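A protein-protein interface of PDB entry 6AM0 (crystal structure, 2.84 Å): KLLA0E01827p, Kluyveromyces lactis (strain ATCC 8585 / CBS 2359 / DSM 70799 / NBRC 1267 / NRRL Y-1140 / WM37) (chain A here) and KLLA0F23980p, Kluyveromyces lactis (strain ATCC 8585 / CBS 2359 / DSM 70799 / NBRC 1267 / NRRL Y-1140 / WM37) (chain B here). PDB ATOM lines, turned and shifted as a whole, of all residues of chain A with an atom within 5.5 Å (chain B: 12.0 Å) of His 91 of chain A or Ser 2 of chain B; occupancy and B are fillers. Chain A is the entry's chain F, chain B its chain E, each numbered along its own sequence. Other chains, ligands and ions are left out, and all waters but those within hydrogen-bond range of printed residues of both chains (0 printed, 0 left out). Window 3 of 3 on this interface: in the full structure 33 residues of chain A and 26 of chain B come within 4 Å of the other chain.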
ATOM      1  N   THR A  89     -15.369  23.290  20.345  1.00  0.00           N
ATOM      2  CA  THR A  89     -16.214  22.187  20.759  1.00  0.00           C
ATOM      3  C   THR A  89     -17.385  22.037  19.793  1.00  0.00           C
ATOM      4  O   THR A  89     -17.935  23.045  19.335  1.00  0.00           O
ATOM      5  CB  THR A  89     -16.728  22.441  22.197  1.00  0.00           C
ATOM      6  OG1 THR A  89     -15.653  22.262  23.130  1.00  0.00           O
ATOM      7  CG2 THR A  89     -17.887  21.526  22.572  1.00  0.00           C
ATOM      8  N   PRO A  90     -17.769  20.809  19.441  1.00  0.00           N
ATOM      9  CA  PRO A  90     -18.862  20.620  18.479  1.00  0.00           C
ATOM     10  C   PRO A  90     -20.191  21.120  19.025  1.00  0.00           C
ATOM     11  O   PRO A  90     -20.351  21.401  20.213  1.00  0.00           O
ATOM     12  CB  PRO A  90     -18.892  19.103  18.273  1.00  0.00           C
ATOM     13  CG  PRO A  90     -18.298  18.549  19.532  1.00  0.00           C
ATOM     14  CD  PRO A  90     -17.209  19.519  19.884  1.00  0.00           C
ATOM     15  N   HIS A  91     -21.165  21.224  18.123  1.00  0.00           N
ATOM     16  CA  HIS A  91     -22.522  21.577  18.524  1.00  0.00           C
ATOM     17  C   HIS A  91     -23.198  20.323  19.061  1.00  0.00           C
ATOM     18  O   HIS A  91     -23.439  19.371  18.310  1.00  0.00           O
ATOM     19  CB  HIS A  91     -23.306  22.171  17.355  1.00  0.00           C
ATOM     20  CG  HIS A  91     -24.670  22.664  17.733  1.00  0.00           C
ATOM     21  ND1 HIS A  91     -25.682  21.819  18.138  1.00  0.00           N
ATOM     22  CD2 HIS A  91     -25.192  23.914  17.763  1.00  0.00           C
ATOM     23  CE1 HIS A  91     -26.765  22.528  18.406  1.00  0.00           C
ATOM     24  NE2 HIS A  91     -26.495  23.801  18.185  1.00  0.00           N
ATOM     25  N   VAL A  92     -23.486  20.311  20.361  1.00  0.00           N
ATOM     26  CA  VAL A  92     -24.226  19.199  20.945  1.00  0.00           C
ATOM     27  C   VAL A  92     -25.650  19.232  20.403  1.00  0.00           C
ATOM     28  O   VAL A  92     -26.343  20.250  20.506  1.00  0.00           O
ATOM     29  CB  VAL A  92     -24.202  19.267  22.476  1.00  0.00           C
ATOM     30  CG1 VAL A  92     -25.079  18.176  23.062  1.00  0.00           C
ATOM     31  CG2 VAL A  92     -22.775  19.132  22.986  1.00  0.00           C
ATOM     32  N   LEU A  93     -26.083  18.119  19.812  1.00  0.00           N
ATOM     33  CA  LEU A  93     -27.393  18.068  19.177  1.00  0.00           C
ATOM     34  C   LEU A  93     -28.506  18.237  20.201  1.00  0.00           C
ATOM     35  O   LEU A  93     -28.480  17.644  21.283  1.00  0.00           O
ATOM     36  CB  LEU A  93     -27.576  16.743  18.435  1.00  0.00           C
ATOM     37  CG  LEU A  93     -26.781  16.497  17.152  1.00  0.00           C
ATOM     38  CD1 LEU A  93     -26.924  15.046  16.714  1.00  0.00           C
ATOM     39  CD2 LEU A  93     -27.246  17.433  16.054  1.00  0.00           C
ATOM     40  N   THR A  94     -29.488  19.057  19.851  1.00  0.00           N
ATOM     41  CA  THR A  94     -30.701  19.214  20.635  1.00  0.00           C
ATOM     42  C   THR A  94     -31.894  18.710  19.836  1.00  0.00           C
ATOM     43  O   THR A  94     -31.788  18.380  18.650  1.00  0.00           O
ATOM     44  CB  THR A  94     -30.911  20.678  21.039  1.00  0.00           C
ATOM     45  OG1 THR A  94     -30.872  21.507  19.869  1.00  0.00           O
ATOM     46  CG2 THR A  94     -29.832  21.122  22.014  1.00  0.00           C
ATOM     47  N   SER A 115     -18.059  11.885  20.403  1.00  0.00           N
ATOM     48  CA  SER A 115     -19.370  11.391  20.015  1.00  0.00           C
ATOM     49  C   SER A 115     -19.749  11.915  18.643  1.00  0.00           C
ATOM     50  O   SER A 115     -19.606  13.110  18.366  1.00  0.00           O
ATOM     51  CB  SER A 115     -20.433  11.805  21.036  1.00  0.00           C
ATOM     52  OG  SER A 115     -21.693  11.942  20.407  1.00  0.00           O
ATOM     53  N   LEU A 116     -20.237  11.017  17.793  1.00  0.00           N
ATOM     54  CA  LEU A 116     -20.829  11.389  16.517  1.00  0.00           C
ATOM     55  C   LEU A 116     -22.144  10.649  16.356  1.00  0.00           C
ATOM     56  O   LEU A 116     -22.217   9.450  16.630  1.00  0.00           O
ATOM     57  CB  LEU A 116     -19.904  11.056  15.345  1.00  0.00           C
ATOM     58  CG  LEU A 116     -18.796  12.056  15.026  1.00  0.00           C
ATOM     59  CD1 LEU A 116     -18.199  11.730  13.669  1.00  0.00           C
ATOM     60  CD2 LEU A 116     -19.333  13.478  15.060  1.00  0.00           C
ATOM     61  N   ALA A 117     -23.179  11.353  15.926  1.00  0.00           N
ATOM     62  CA  ALA A 117     -24.429  10.701  15.572  1.00  0.00           C
ATOM     63  C   ALA A 117     -24.405  10.323  14.097  1.00  0.00           C
ATOM     64  O   ALA A 117     -23.791  11.005  13.273  1.00  0.00           O
ATOM     65  CB  ALA A 117     -25.621  11.611  15.867  1.00  0.00           C
ATOM     66  N   LYS A 156     -24.007  18.313  11.012  1.00  0.00           N
ATOM     67  CA  LYS A 156     -23.939  19.759  11.173  1.00  0.00           C
ATOM     68  C   LYS A 156     -22.720  20.354  10.477  1.00  0.00           C
ATOM     69  O   LYS A 156     -22.281  21.453  10.834  1.00  0.00           O
ATOM     70  CB  LYS A 156     -23.948  20.135  12.654  1.00  0.00           C
ATOM     71  CG  LYS A 156     -25.121  19.548  13.411  1.00  0.00           C
ATOM     72  CD  LYS A 156     -25.296  20.189  14.773  1.00  0.00           C
ATOM     73  CE  LYS A 156     -25.970  21.546  14.662  1.00  0.00           C
ATOM     74  NZ  LYS A 156     -27.055  21.710  15.672  1.00  0.00           N
ATOM     75  N   GLU A 158     -19.578  19.777  10.487  1.00  0.00           N
ATOM     76  CA  GLU A 158     -18.235  19.644  11.031  1.00  0.00           C
ATOM     77  C   GLU A 158     -17.480  18.571  10.255  1.00  0.00           C
ATOM     78  O   GLU A 158     -18.066  17.600   9.769  1.00  0.00           O
ATOM     79  CB  GLU A 158     -18.284  19.279  12.515  1.00  0.00           C
ATOM     80  CG  GLU A 158     -19.139  20.202  13.364  1.00  0.00           C
ATOM     81  CD  GLU A 158     -19.553  19.567  14.680  1.00  0.00           C
ATOM     82  OE1 GLU A 158     -19.399  18.334  14.827  1.00  0.00           O
ATOM     83  OE2 GLU A 158     -20.037  20.302  15.567  1.00  0.00           O
ATOM     84  N   SER B   2     -21.167  15.721  19.543  1.00  0.00           N
ATOM     85  CA  SER B   2     -22.339  15.749  18.678  1.00  0.00           C
ATOM     86  C   SER B   2     -23.572  15.320  19.468  1.00  0.00           C
ATOM     87  O   SER B   2     -24.540  16.070  19.573  1.00  0.00           O
ATOM     88  CB  SER B   2     -22.133  14.848  17.454  1.00  0.00           C
ATOM     89  OG  SER B   2     -23.145  15.040  16.474  1.00  0.00           O
ATOM     90  N   LEU B   3     -23.525  14.079  20.052  1.00  0.00           N
ATOM     91  CA  LEU B   3     -24.641  13.612  20.870  1.00  0.00           C
ATOM     92  C   LEU B   3     -24.445  14.022  22.327  1.00  0.00           C
ATOM     93  O   LEU B   3     -23.330  13.940  22.852  1.00  0.00           O
ATOM     94  CB  LEU B   3     -24.776  12.095  20.797  1.00  0.00           C
ATOM     95  CG  LEU B   3     -25.557  11.465  19.644  1.00  0.00           C
ATOM     96  CD1 LEU B   3     -25.257   9.978  19.583  1.00  0.00           C
ATOM     97  CD2 LEU B   3     -27.048  11.698  19.820  1.00  0.00           C
ATOM     98  N   PRO B   4     -25.511  14.458  23.000  1.00  0.00           N
ATOM     99  CA  PRO B   4     -25.401  14.766  24.433  1.00  0.00           C
ATOM    100  C   PRO B   4     -25.136  13.523  25.264  1.00  0.00           C
ATOM    101  O   PRO B   4     -25.987  12.634  25.349  1.00  0.00           O
ATOM    102  CB  PRO B   4     -26.766  15.383  24.763  1.00  0.00           C
ATOM    103  CG  PRO B   4     -27.686  14.844  23.725  1.00  0.00           C
ATOM    104  CD  PRO B   4     -26.861  14.728  22.477  1.00  0.00           C
ATOM    105  N   LEU B   5     -23.963  13.449  25.882  1.00  0.00           N
ATOM    106  CA  LEU B   5     -23.595  12.331  26.736  1.00  0.00           C
ATOM    107  C   LEU B   5     -23.669  12.756  28.197  1.00  0.00           C
ATOM    108  O   LEU B   5     -23.276  13.871  28.551  1.00  0.00           O
ATOM    109  CB  LEU B   5     -22.185  11.824  26.410  1.00  0.00           C
ATOM    110  CG  LEU B   5     -21.926  11.335  24.982  1.00  0.00           C
ATOM    111  CD1 LEU B   5     -20.491  10.844  24.828  1.00  0.00           C
ATOM    112  CD2 LEU B   5     -22.912  10.242  24.598  1.00  0.00           C
ATOM    113  N   LEU B   6     -24.181  11.864  29.040  1.00  0.00           N
ATOM    114  CA  LEU B   6     -24.230  12.135  30.465  1.00  0.00           C
ATOM    115  C   LEU B   6     -22.826  12.070  31.062  1.00  0.00           C
ATOM    116  O   LEU B   6     -21.849  11.707  30.399  1.00  0.00           O
ATOM    117  CB  LEU B   6     -25.153  11.142  31.173  1.00  0.00           C
ATOM    118  CG  LEU B   6     -26.556  10.979  30.586  1.00  0.00           C
ATOM    119  CD1 LEU B   6     -27.394  10.040  31.443  1.00  0.00           C
ATOM    120  CD2 LEU B   6     -27.235  12.331  30.437  1.00  0.00           C
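The backbone NH (N) of Ser 2 of chain B lies close to the backbone carbonyl oxygen (O) of Ser 115 of chain A, 3.3 Å away.
The side-chain hydroxyl (OG) of Ser 115 of chain A is in hydrogen-bond range of the backbone NH (N) of Leu 3 of chain B.
The backbone carbonyl oxygen (O) of Ser 2 of chain B is in hydrogen-bond range of the backbone NH (N) of Leu 93 of chain A (2.6 Å).
Hydrophobic or aromatic side chains of chain B within 4 Å of the printed part of chain A: Leu 3, Pro 4 and Leu 5.
Of the 11 printed residues of chain A, 6 touch a printed residue of chain B.
Among the printed residues, 11 pairs touch across the chains.
Among the printed residues, no Asp or Glu carboxylate lies within 4 Å of a Lys or Arg side-chain nitrogen of the other chain.
His 91 of chain A touches one residue of chain B.
No residue of chain B comes within 4 Å of Thr 89 of chain A.
No residue of chain B comes within 4 Å of Pro 90 of chain A.
Of chain B, only Ser 2 (3.4 Å) and Pro 4 (3.7 Å) come within 4 Å of Val 92 of chain A.
Of chain B, only Ser 2 (2.6 Å) and Pro 4 (3.5 Å) come within 4 Å of Leu 93 of chain A.
No residue of chain B comes within 4 Å of Thr 94 of chain A.
Printed residues of chain B within 4 Å of Leu 116 of chain A: Ser 2.
Ala 117 of chain A touches just these residues of chain B: Ser 2 (3.7 Å) and Leu 3 (3.8 Å).
Of the printed residues of chain A, Pro 4 of chain B touches Val 92 (3.7 Å) and Leu 93 (3.5 Å).
Printed residues of chain A within 4 Å of Leu 5 of chain B: Ser 115 (3.9 Å).
Leu 6 of chain B touches none of the printed residues of chain A.
The nearest residue of chain B that does not touch His 91 of chain A is Leu 3 of chain B (5.6 Å).
The nearest residue of chain A that does not touch Ser 2 of chain B is Pro 90 of chain A (4.03 Å).
The nearest printed residue of chain A that does not touch Leu 5 of chain B is Val 92 of chain A (5.6 Å).
ND1 of His 91 of chain A is in hydrogen-bond range of NZ of Lys 156 of chain A (2.8 Å).
The backbone NH of His 91 of chain A lies within hydrogen-bond range of the side-chain carboxylate of Glu 158 of chain A.
Among the printed residues, pairs that only touch across the chains: His 91 of chain A with Ser 2 of chain B, Val 92 of chain A with Ser 2 of chain B, Val 92 of chain A with Pro 4 of chain B, Leu 93 of chain A with Pro 4 of chain B, Ser 115 of chain A with Leu 5 of chain B, Leu 116 of chain A with Ser 2 of chain B, Ala 117 of chain A with Ser 2 of chain B and Ala 117 of chain A with Leu 3 of chain B.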
